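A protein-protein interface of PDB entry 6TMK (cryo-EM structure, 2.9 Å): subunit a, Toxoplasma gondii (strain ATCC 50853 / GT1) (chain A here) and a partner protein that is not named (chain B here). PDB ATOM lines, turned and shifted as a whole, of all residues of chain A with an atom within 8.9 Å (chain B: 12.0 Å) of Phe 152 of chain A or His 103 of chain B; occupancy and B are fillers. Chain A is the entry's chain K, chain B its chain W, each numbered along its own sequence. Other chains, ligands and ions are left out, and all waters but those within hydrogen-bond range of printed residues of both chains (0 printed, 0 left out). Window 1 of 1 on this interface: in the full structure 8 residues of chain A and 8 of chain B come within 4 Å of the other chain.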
ATOM      1  N   THR A 145      -1.202  31.438   5.444  1.00  0.00           N
ATOM      2  CA  THR A 145      -0.132  30.480   5.186  1.00  0.00           C
ATOM      3  C   THR A 145       0.127  29.610   6.408  1.00  0.00           C
ATOM      4  O   THR A 145       0.336  28.397   6.290  1.00  0.00           O
ATOM      5  CB  THR A 145       1.138  31.226   4.777  1.00  0.00           C
ATOM      6  OG1 THR A 145       0.820  32.217   3.795  1.00  0.00           O
ATOM      7  CG2 THR A 145       2.153  30.273   4.203  1.00  0.00           C
ATOM      8  N   PHE A 146       0.098  30.214   7.595  1.00  0.00           N
ATOM      9  CA  PHE A 146       0.367  29.481   8.823  1.00  0.00           C
ATOM     10  C   PHE A 146      -0.692  28.421   9.078  1.00  0.00           C
ATOM     11  O   PHE A 146      -0.371  27.293   9.463  1.00  0.00           O
ATOM     12  CB  PHE A 146       0.452  30.457   9.992  1.00  0.00           C
ATOM     13  CG  PHE A 146       0.664  29.800  11.316  1.00  0.00           C
ATOM     14  CD1 PHE A 146       1.917  29.378  11.701  1.00  0.00           C
ATOM     15  CD2 PHE A 146      -0.392  29.612  12.181  1.00  0.00           C
ATOM     16  CE1 PHE A 146       2.110  28.777  12.919  1.00  0.00           C
ATOM     17  CE2 PHE A 146      -0.205  29.012  13.397  1.00  0.00           C
ATOM     18  CZ  PHE A 146       1.046  28.593  13.768  1.00  0.00           C
ATOM     19  N   LEU A 147      -1.964  28.764   8.867  1.00  0.00           N
ATOM     20  CA  LEU A 147      -3.018  27.774   9.053  1.00  0.00           C
ATOM     21  C   LEU A 147      -2.967  26.701   7.973  1.00  0.00           C
ATOM     22  O   LEU A 147      -3.212  25.524   8.252  1.00  0.00           O
ATOM     23  CB  LEU A 147      -4.378  28.463   9.063  1.00  0.00           C
ATOM     24  CG  LEU A 147      -4.588  29.472  10.188  1.00  0.00           C
ATOM     25  CD1 LEU A 147      -5.829  30.295   9.934  1.00  0.00           C
ATOM     26  CD2 LEU A 147      -4.674  28.783  11.524  1.00  0.00           C
ATOM     27  N   LEU A 148      -2.646  27.082   6.737  1.00  0.00           N
ATOM     28  CA  LEU A 148      -2.538  26.101   5.665  1.00  0.00           C
ATOM     29  C   LEU A 148      -1.376  25.144   5.889  1.00  0.00           C
ATOM     30  O   LEU A 148      -1.399  24.019   5.380  1.00  0.00           O
ATOM     31  CB  LEU A 148      -2.384  26.801   4.317  1.00  0.00           C
ATOM     32  CG  LEU A 148      -3.646  27.110   3.505  1.00  0.00           C
ATOM     33  CD1 LEU A 148      -4.393  25.838   3.168  1.00  0.00           C
ATOM     34  CD2 LEU A 148      -4.559  28.071   4.230  1.00  0.00           C
ATOM     35  N   ASN A 149      -0.352  25.567   6.626  1.00  0.00           N
ATOM     36  CA  ASN A 149       0.781  24.683   6.872  1.00  0.00           C
ATOM     37  C   ASN A 149       0.481  23.571   7.869  1.00  0.00           C
ATOM     38  O   ASN A 149       1.388  22.792   8.175  1.00  0.00           O
ATOM     39  CB  ASN A 149       1.979  25.484   7.380  1.00  0.00           C
ATOM     40  CG  ASN A 149       2.592  26.367   6.317  1.00  0.00           C
ATOM     41  OD1 ASN A 149       2.826  27.553   6.542  1.00  0.00           O
ATOM     42  ND2 ASN A 149       2.883  25.790   5.164  1.00  0.00           N
ATOM     43  N   PHE A 150      -0.740  23.471   8.389  1.00  0.00           N
ATOM     44  CA  PHE A 150      -1.073  22.398   9.318  1.00  0.00           C
ATOM     45  C   PHE A 150      -1.268  21.055   8.629  1.00  0.00           C
ATOM     46  O   PHE A 150      -1.390  20.037   9.317  1.00  0.00           O
ATOM     47  CB  PHE A 150      -2.328  22.751  10.112  1.00  0.00           C
ATOM     48  CG  PHE A 150      -2.046  23.473  11.389  1.00  0.00           C
ATOM     49  CD1 PHE A 150      -1.452  24.716  11.379  1.00  0.00           C
ATOM     50  CD2 PHE A 150      -2.367  22.902  12.604  1.00  0.00           C
ATOM     51  CE1 PHE A 150      -1.189  25.378  12.552  1.00  0.00           C
ATOM     52  CE2 PHE A 150      -2.102  23.562  13.781  1.00  0.00           C
ATOM     53  CZ  PHE A 150      -1.512  24.801  13.754  1.00  0.00           C
ATOM     54  N   ARG A 151      -1.302  21.028   7.298  1.00  0.00           N
ATOM     55  CA  ARG A 151      -1.455  19.774   6.572  1.00  0.00           C
ATOM     56  C   ARG A 151      -0.244  18.866   6.735  1.00  0.00           C
ATOM     57  O   ARG A 151      -0.366  17.637   6.621  1.00  0.00           O
ATOM     58  CB  ARG A 151      -1.704  20.081   5.099  1.00  0.00           C
ATOM     59  CG  ARG A 151      -0.552  20.777   4.421  1.00  0.00           C
ATOM     60  CD  ARG A 151      -0.936  21.259   3.047  1.00  0.00           C
ATOM     61  NE  ARG A 151       0.184  21.862   2.334  1.00  0.00           N
ATOM     62  CZ  ARG A 151       0.599  23.110   2.515  1.00  0.00           C
ATOM     63  NH1 ARG A 151       1.622  23.573   1.820  1.00  0.00           N
ATOM     64  NH2 ARG A 151      -0.005  23.897   3.390  1.00  0.00           N
ATOM     65  N   PHE A 152       0.928  19.448   6.978  1.00  0.00           N
ATOM     66  CA  PHE A 152       2.139  18.647   7.075  1.00  0.00           C
ATOM     67  C   PHE A 152       2.091  17.730   8.286  1.00  0.00           C
ATOM     68  O   PHE A 152       2.580  16.597   8.234  1.00  0.00           O
ATOM     69  CB  PHE A 152       3.357  19.558   7.140  1.00  0.00           C
ATOM     70  CG  PHE A 152       3.638  20.278   5.861  1.00  0.00           C
ATOM     71  CD1 PHE A 152       3.327  21.613   5.723  1.00  0.00           C
ATOM     72  CD2 PHE A 152       4.209  19.618   4.796  1.00  0.00           C
ATOM     73  CE1 PHE A 152       3.583  22.274   4.552  1.00  0.00           C
ATOM     74  CE2 PHE A 152       4.467  20.275   3.621  1.00  0.00           C
ATOM     75  CZ  PHE A 152       4.153  21.605   3.498  1.00  0.00           C
ATOM     76  N   TYR A 153       1.491  18.194   9.383  1.00  0.00           N
ATOM     77  CA  TYR A 153       1.358  17.343  10.557  1.00  0.00           C
ATOM     78  C   TYR A 153       0.500  16.125  10.251  1.00  0.00           C
ATOM     79  O   TYR A 153       0.824  15.005  10.659  1.00  0.00           O
ATOM     80  CB  TYR A 153       0.743  18.140  11.705  1.00  0.00           C
ATOM     81  CG  TYR A 153       1.492  19.392  12.077  1.00  0.00           C
ATOM     82  CD1 TYR A 153       2.766  19.334  12.610  1.00  0.00           C
ATOM     83  CD2 TYR A 153       0.918  20.635  11.895  1.00  0.00           C
ATOM     84  CE1 TYR A 153       3.443  20.481  12.951  1.00  0.00           C
ATOM     85  CE2 TYR A 153       1.586  21.781  12.231  1.00  0.00           C
ATOM     86  CZ  TYR A 153       2.847  21.704  12.756  1.00  0.00           C
ATOM     87  OH  TYR A 153       3.506  22.861  13.089  1.00  0.00           O
ATOM     88  N   PHE A 154      -0.604  16.331   9.533  1.00  0.00           N
ATOM     89  CA  PHE A 154      -1.480  15.225   9.179  1.00  0.00           C
ATOM     90  C   PHE A 154      -0.766  14.231   8.272  1.00  0.00           C
ATOM     91  O   PHE A 154      -0.844  13.012   8.482  1.00  0.00           O
ATOM     92  CB  PHE A 154      -2.751  15.768   8.536  1.00  0.00           C
ATOM     93  CG  PHE A 154      -3.593  16.559   9.486  1.00  0.00           C
ATOM     94  CD1 PHE A 154      -4.341  15.928  10.459  1.00  0.00           C
ATOM     95  CD2 PHE A 154      -3.623  17.936   9.418  1.00  0.00           C
ATOM     96  CE1 PHE A 154      -5.104  16.655  11.340  1.00  0.00           C
ATOM     97  CE2 PHE A 154      -4.385  18.667  10.296  1.00  0.00           C
ATOM     98  CZ  PHE A 154      -5.127  18.027  11.257  1.00  0.00           C
ATOM     99  N   MET A 155      -0.050  14.738   7.269  1.00  0.00           N
ATOM    100  CA  MET A 155       0.728  13.865   6.395  1.00  0.00           C
ATOM    101  C   MET A 155       1.730  13.044   7.199  1.00  0.00           C
ATOM    102  O   MET A 155       1.851  11.823   7.017  1.00  0.00           O
ATOM    103  CB  MET A 155       1.452  14.694   5.340  1.00  0.00           C
ATOM    104  CG  MET A 155       0.538  15.372   4.345  1.00  0.00           C
ATOM    105  SD  MET A 155       1.361  16.682   3.423  1.00  0.00           S
ATOM    106  CE  MET A 155       0.020  17.240   2.378  1.00  0.00           C
ATOM    107  N   TYR A 156       2.460  13.705   8.097  1.00  0.00           N
ATOM    108  CA  TYR A 156       3.501  13.024   8.853  1.00  0.00           C
ATOM    109  C   TYR A 156       2.913  11.959   9.763  1.00  0.00           C
ATOM    110  O   TYR A 156       3.461  10.856   9.866  1.00  0.00           O
ATOM    111  CB  TYR A 156       4.298  14.030   9.680  1.00  0.00           C
ATOM    112  CG  TYR A 156       5.087  15.033   8.878  1.00  0.00           C
ATOM    113  CD1 TYR A 156       5.587  14.719   7.627  1.00  0.00           C
ATOM    114  CD2 TYR A 156       5.351  16.292   9.387  1.00  0.00           C
ATOM    115  CE1 TYR A 156       6.308  15.634   6.902  1.00  0.00           C
ATOM    116  CE2 TYR A 156       6.072  17.212   8.670  1.00  0.00           C
ATOM    117  CZ  TYR A 156       6.550  16.879   7.428  1.00  0.00           C
ATOM    118  OH  TYR A 156       7.272  17.799   6.706  1.00  0.00           O
ATOM    119  N   MET A 157       1.804  12.263  10.437  1.00  0.00           N
ATOM    120  CA  MET A 157       1.217  11.266  11.322  1.00  0.00           C
ATOM    121  C   MET A 157       0.663  10.090  10.531  1.00  0.00           C
ATOM    122  O   MET A 157       0.755   8.941  10.978  1.00  0.00           O
ATOM    123  CB  MET A 157       0.124  11.900  12.176  1.00  0.00           C
ATOM    124  CG  MET A 157      -1.049  12.412  11.390  1.00  0.00           C
ATOM    125  SD  MET A 157      -2.395  12.991  12.439  1.00  0.00           S
ATOM    126  CE  MET A 157      -1.544  14.218  13.420  1.00  0.00           C
ATOM    127  N   ALA A 158       0.103  10.344   9.347  1.00  0.00           N
ATOM    128  CA  ALA A 158      -0.368   9.244   8.515  1.00  0.00           C
ATOM    129  C   ALA A 158       0.782   8.316   8.148  1.00  0.00           C
ATOM    130  O   ALA A 158       0.691   7.088   8.307  1.00  0.00           O
ATOM    131  CB  ALA A 158      -1.040   9.794   7.263  1.00  0.00           C
ATOM    132  N   ARG A 159       1.882   8.895   7.668  1.00  0.00           N
ATOM    133  CA  ARG A 159       3.047   8.095   7.307  1.00  0.00           C
ATOM    134  C   ARG A 159       3.568   7.312   8.502  1.00  0.00           C
ATOM    135  O   ARG A 159       3.885   6.119   8.393  1.00  0.00           O
ATOM    136  CB  ARG A 159       4.138   9.002   6.748  1.00  0.00           C
ATOM    137  CG  ARG A 159       3.916   9.398   5.313  1.00  0.00           C
ATOM    138  CD  ARG A 159       4.593  10.710   4.979  1.00  0.00           C
ATOM    139  NE  ARG A 159       6.026  10.684   5.245  1.00  0.00           N
ATOM    140  CZ  ARG A 159       6.908   9.990   4.534  1.00  0.00           C
ATOM    141  NH1 ARG A 159       6.512   9.251   3.508  1.00  0.00           N
ATOM    142  NH2 ARG A 159       8.190  10.033   4.850  1.00  0.00           N
ATOM    143  N   THR A 160       3.656   7.971   9.655  1.00  0.00           N
ATOM    144  CA  THR A 160       4.205   7.336  10.843  1.00  0.00           C
ATOM    145  C   THR A 160       3.349   6.155  11.275  1.00  0.00           C
ATOM    146  O   THR A 160       3.867   5.072  11.576  1.00  0.00           O
ATOM    147  CB  THR A 160       4.320   8.370  11.960  1.00  0.00           C
ATOM    148  OG1 THR A 160       5.161   9.445  11.528  1.00  0.00           O
ATOM    149  CG2 THR A 160       4.900   7.762  13.199  1.00  0.00           C
ATOM    150  N   PRO B  89       8.975  17.255  21.403  1.00  0.00           N
ATOM    151  CA  PRO B  89       9.961  18.153  20.811  1.00  0.00           C
ATOM    152  C   PRO B  89      10.657  18.984  21.871  1.00  0.00           C
ATOM    153  O   PRO B  89      10.082  19.339  22.902  1.00  0.00           O
ATOM    154  CB  PRO B  89       9.109  19.024  19.886  1.00  0.00           C
ATOM    155  CG  PRO B  89       7.835  19.129  20.622  1.00  0.00           C
ATOM    156  CD  PRO B  89       7.608  17.742  21.167  1.00  0.00           C
ATOM    157  N   ASN B  90      11.920  19.291  21.605  1.00  0.00           N
ATOM    158  CA  ASN B  90      12.713  20.104  22.517  1.00  0.00           C
ATOM    159  C   ASN B  90      12.286  21.560  22.404  1.00  0.00           C
ATOM    160  O   ASN B  90      12.541  22.215  21.389  1.00  0.00           O
ATOM    161  CB  ASN B  90      14.195  19.946  22.213  1.00  0.00           C
ATOM    162  CG  ASN B  90      15.056  20.123  23.431  1.00  0.00           C
ATOM    163  OD1 ASN B  90      14.667  20.785  24.390  1.00  0.00           O
ATOM    164  ND2 ASN B  90      16.238  19.538  23.403  1.00  0.00           N
ATOM    165  N   LEU B  91      11.628  22.060  23.443  1.00  0.00           N
ATOM    166  CA  LEU B  91      11.216  23.450  23.511  1.00  0.00           C
ATOM    167  C   LEU B  91      12.217  24.319  24.252  1.00  0.00           C
ATOM    168  O   LEU B  91      12.049  25.541  24.284  1.00  0.00           O
ATOM    169  CB  LEU B  91       9.858  23.553  24.205  1.00  0.00           C
ATOM    170  CG  LEU B  91       8.789  22.598  23.692  1.00  0.00           C
ATOM    171  CD1 LEU B  91       7.538  22.731  24.514  1.00  0.00           C
ATOM    172  CD2 LEU B  91       8.503  22.877  22.242  1.00  0.00           C
ATOM    173  N   PHE B  94      15.433  27.043  20.584  1.00  0.00           N
ATOM    174  CA  PHE B  94      14.652  27.610  19.486  1.00  0.00           C
ATOM    175  C   PHE B  94      13.179  27.721  19.861  1.00  0.00           C
ATOM    176  O   PHE B  94      12.291  27.429  19.060  1.00  0.00           O
ATOM    177  CB  PHE B  94      14.824  26.799  18.204  1.00  0.00           C
ATOM    178  CG  PHE B  94      16.243  26.455  17.890  1.00  0.00           C
ATOM    179  CD1 PHE B  94      17.228  27.416  17.955  1.00  0.00           C
ATOM    180  CD2 PHE B  94      16.593  25.174  17.519  1.00  0.00           C
ATOM    181  CE1 PHE B  94      18.529  27.105  17.664  1.00  0.00           C
ATOM    182  CE2 PHE B  94      17.894  24.863  17.227  1.00  0.00           C
ATOM    183  CZ  PHE B  94      18.863  25.831  17.297  1.00  0.00           C
ATOM    184  N   THR B  95      12.918  28.147  21.096  1.00  0.00           N
ATOM    185  CA  THR B  95      11.547  28.217  21.581  1.00  0.00           C
ATOM    186  C   THR B  95      10.728  29.213  20.774  1.00  0.00           C
ATOM    187  O   THR B  95       9.571  28.948  20.431  1.00  0.00           O
ATOM    188  CB  THR B  95      11.544  28.607  23.057  1.00  0.00           C
ATOM    189  OG1 THR B  95      12.493  27.809  23.768  1.00  0.00           O
ATOM    190  CG2 THR B  95      10.177  28.405  23.660  1.00  0.00           C
ATOM    191  N   ARG B  96      11.311  30.368  20.464  1.00  0.00           N
ATOM    192  CA  ARG B  96      10.570  31.416  19.774  1.00  0.00           C
ATOM    193  C   ARG B  96      10.172  31.011  18.360  1.00  0.00           C
ATOM    194  O   ARG B  96       9.152  31.483  17.849  1.00  0.00           O
ATOM    195  CB  ARG B  96      11.408  32.686  19.751  1.00  0.00           C
ATOM    196  CG  ARG B  96      10.616  33.945  19.641  1.00  0.00           C
ATOM    197  CD  ARG B  96      11.518  35.144  19.551  1.00  0.00           C
ATOM    198  NE  ARG B  96      12.156  35.254  18.246  1.00  0.00           N
ATOM    199  CZ  ARG B  96      12.449  36.404  17.651  1.00  0.00           C
ATOM    200  NH1 ARG B  96      12.185  37.556  18.236  1.00  0.00           N
ATOM    201  NH2 ARG B  96      13.025  36.399  16.466  1.00  0.00           N
ATOM    202  N   ALA B  97      10.952  30.147  17.715  1.00  0.00           N
ATOM    203  CA  ALA B  97      10.735  29.763  16.329  1.00  0.00           C
ATOM    204  C   ALA B  97       9.941  28.471  16.172  1.00  0.00           C
ATOM    205  O   ALA B  97       9.677  28.056  15.038  1.00  0.00           O
ATOM    206  CB  ALA B  97      12.077  29.624  15.621  1.00  0.00           C
ATOM    207  N   PHE B  98       9.557  27.836  17.274  1.00  0.00           N
ATOM    208  CA  PHE B  98       8.973  26.500  17.199  1.00  0.00           C
ATOM    209  C   PHE B  98       7.706  26.455  16.359  1.00  0.00           C
ATOM    210  O   PHE B  98       7.591  25.558  15.506  1.00  0.00           O
ATOM    211  CB  PHE B  98       8.726  25.986  18.619  1.00  0.00           C
ATOM    212  CG  PHE B  98       7.870  24.766  18.679  1.00  0.00           C
ATOM    213  CD1 PHE B  98       8.379  23.536  18.325  1.00  0.00           C
ATOM    214  CD2 PHE B  98       6.557  24.846  19.090  1.00  0.00           C
ATOM    215  CE1 PHE B  98       7.598  22.416  18.378  1.00  0.00           C
ATOM    216  CE2 PHE B  98       5.774  23.727  19.143  1.00  0.00           C
ATOM    217  CZ  PHE B  98       6.293  22.511  18.789  1.00  0.00           C
ATOM    218  N   PRO B  99       6.746  27.366  16.515  1.00  0.00           N
ATOM    219  CA  PRO B  99       5.582  27.353  15.617  1.00  0.00           C
ATOM    220  C   PRO B  99       5.939  27.563  14.163  1.00  0.00           C
ATOM    221  O   PRO B  99       5.151  27.192  13.285  1.00  0.00           O
ATOM    222  CB  PRO B  99       4.719  28.504  16.145  1.00  0.00           C
ATOM    223  CG  PRO B  99       5.207  28.772  17.503  1.00  0.00           C
ATOM    224  CD  PRO B  99       6.642  28.431  17.519  1.00  0.00           C
ATOM    225  N   PHE B 100       7.098  28.143  13.878  1.00  0.00           N
ATOM    226  CA  PHE B 100       7.473  28.475  12.515  1.00  0.00           C
ATOM    227  C   PHE B 100       8.297  27.395  11.832  1.00  0.00           C
ATOM    228  O   PHE B 100       8.320  27.349  10.598  1.00  0.00           O
ATOM    229  CB  PHE B 100       8.239  29.795  12.500  1.00  0.00           C
ATOM    230  CG  PHE B 100       7.522  30.915  13.189  1.00  0.00           C
ATOM    231  CD1 PHE B 100       6.599  31.681  12.510  1.00  0.00           C
ATOM    232  CD2 PHE B 100       7.768  31.200  14.514  1.00  0.00           C
ATOM    233  CE1 PHE B 100       5.942  32.705  13.139  1.00  0.00           C
ATOM    234  CE2 PHE B 100       7.110  32.225  15.144  1.00  0.00           C
ATOM    235  CZ  PHE B 100       6.197  32.977  14.456  1.00  0.00           C
ATOM    236  N   TYR B 101       8.976  26.532  12.588  1.00  0.00           N
ATOM    237  CA  TYR B 101       9.742  25.441  11.998  1.00  0.00           C
ATOM    238  C   TYR B 101       9.194  24.059  12.326  1.00  0.00           C
ATOM    239  O   TYR B 101       9.740  23.066  11.836  1.00  0.00           O
ATOM    240  CB  TYR B 101      11.220  25.531  12.409  1.00  0.00           C
ATOM    241  CG  TYR B 101      11.552  25.143  13.829  1.00  0.00           C
ATOM    242  CD1 TYR B 101      11.662  23.817  14.206  1.00  0.00           C
ATOM    243  CD2 TYR B 101      11.819  26.108  14.775  1.00  0.00           C
ATOM    244  CE1 TYR B 101      11.979  23.471  15.495  1.00  0.00           C
ATOM    245  CE2 TYR B 101      12.147  25.770  16.062  1.00  0.00           C
ATOM    246  CZ  TYR B 101      12.222  24.453  16.421  1.00  0.00           C
ATOM    247  OH  TYR B 101      12.548  24.122  17.714  1.00  0.00           O
ATOM    248  N   ALA B 102       8.131  23.962  13.122  1.00  0.00           N
ATOM    249  CA  ALA B 102       7.640  22.654  13.543  1.00  0.00           C
ATOM    250  C   ALA B 102       7.113  21.834  12.372  1.00  0.00           C
ATOM    251  O   ALA B 102       7.135  20.601  12.426  1.00  0.00           O
ATOM    252  CB  ALA B 102       6.551  22.827  14.593  1.00  0.00           C
ATOM    253  N   HIS B 103       6.642  22.489  11.313  1.00  0.00           N
ATOM    254  CA  HIS B 103       6.029  21.807  10.182  1.00  0.00           C
ATOM    255  C   HIS B 103       7.045  21.240   9.201  1.00  0.00           C
ATOM    256  O   HIS B 103       6.653  20.515   8.282  1.00  0.00           O
ATOM    257  CB  HIS B 103       5.071  22.746   9.451  1.00  0.00           C
ATOM    258  CG  HIS B 103       5.743  23.903   8.786  1.00  0.00           C
ATOM    259  ND1 HIS B 103       6.123  25.035   9.472  1.00  0.00           N
ATOM    260  CD2 HIS B 103       6.095  24.109   7.496  1.00  0.00           C
ATOM    261  CE1 HIS B 103       6.684  25.885   8.633  1.00  0.00           C
ATOM    262  NE2 HIS B 103       6.679  25.347   7.428  1.00  0.00           N
ATOM    263  N   THR B 104       8.323  21.549   9.365  1.00  0.00           N
ATOM    264  CA  THR B 104       9.356  21.076   8.461  1.00  0.00           C
ATOM    265  C   THR B 104       9.905  19.737   8.947  1.00  0.00           C
ATOM    266  O   THR B 104       9.677  19.313  10.082  1.00  0.00           O
ATOM    267  CB  THR B 104      10.482  22.098   8.329  1.00  0.00           C
ATOM    268  OG1 THR B 104      11.343  22.019   9.470  1.00  0.00           O
ATOM    269  CG2 THR B 104       9.915  23.490   8.220  1.00  0.00           C
ATOM    270  N   SER B 105      10.643  19.071   8.064  1.00  0.00           N
ATOM    271  CA  SER B 105      11.247  17.777   8.343  1.00  0.00           C
ATOM    272  C   SER B 105      12.761  17.863   8.246  1.00  0.00           C
ATOM    273  O   SER B 105      13.299  18.412   7.279  1.00  0.00           O
ATOM    274  CB  SER B 105      10.729  16.717   7.366  1.00  0.00           C
ATOM    275  OG  SER B 105       9.419  17.024   6.930  1.00  0.00           O
ATOM    276  N   ALA B 106      13.435  17.329   9.259  1.00  0.00           N
ATOM    277  CA  ALA B 106      14.887  17.325   9.319  1.00  0.00           C
ATOM    278  C   ALA B 106      15.432  16.025   8.738  1.00  0.00           C
ATOM    279  O   ALA B 106      15.082  15.637   7.624  1.00  0.00           O
ATOM    280  CB  ALA B 106      15.349  17.487  10.755  1.00  0.00           C
ATOM    281  OXT ALA B 106      16.228  15.330   9.368  1.00  0.00           O
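OH of Tyr 156 of chain A lies within hydrogen-bond range of O of His 103 of chain B, 3.2 Å away.
OH of Tyr 156 of chain A lies close to OG of Ser 105 of chain B, at 2.3 Å.
ND1 of His 103 of chain B sits close to O of Phe 100 of chain B, 3.4 Å away.
OG1 of Thr 104 of chain B is in hydrogen-bond range of O of Tyr 101 of chain B, at 3.0 Å.
O of Thr 145 of chain A sits close to OD1 of Asn 149 of chain A.
The backbone carbonyl oxygen of Tyr 156 of chain A sits at hydrogen-bond distance from the side-chain hydroxyl of Thr 160 of chain A.
Phe 146 of chain A touches Pro 99 of chain B.
Asn 149 of chain A touches His 103 of chain B (O to CB, 3.9 Å).
Phe 152 of chain A touches His 103 of chain B.
Ala 102 of chain B touches Tyr 153 of chain A (CB to OH, 3.4 Å).
OH of Tyr 153 of chain A touches N of His 103 of chain B, at 3.6 Å.
Thr 104 of chain B touches Tyr 156 of chain A.
Of chain B, only His 103 comes within 4 Å of Phe 152 of chain A.
Printed residues of chain B within 4 Å of Asn 149 of chain A: His 103.
No residue of chain B comes within 4 Å of Phe 154 of chain A.
Tyr 156 of chain A touches just these residues of chain B: His 103, Thr 104 and Ser 105.
Of chain A, only Tyr 153 (3.4 Å) comes within 4 Å of Ala 102 of chain B.
Thr 104 of chain B touches one residue of chain A.
Printed residues of chain A within 4 Å of Ser 105 of chain B: Tyr 156 (2.3 Å).
Of the printed residues of chain B, Phe 146 of chain A touches Pro 99.
Printed residues of chain A within 4 Å of Pro 99 of chain B: Phe 146.
Asn 90 of chain B touches none of the printed residues of chain A.
Thr 145 of chain A touches none of the printed residues of chain B.
The nearest residue of chain A that does not touch His 103 of chain B is Phe 150 of chain A (6.0 Å).
Hydrophobic or aromatic side chains of chain A within 4 Å of the printed part of chain B: Phe 146, Phe 152, Tyr 153 and Tyr 156.
Of the 16 printed residues of chain B, 5 touch a printed residue of chain A.
Printed residues of chain B that touch a printed residue of chain A: Pro 99, Ala 102, His 103, Thr 104 and Ser 105.
Among the printed residues, 8 pairs touch across the chains.
Among the printed residues, no Asp or Glu carboxylate lies within 4 Å of a Lys or Arg side-chain nitrogen of the other chain.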
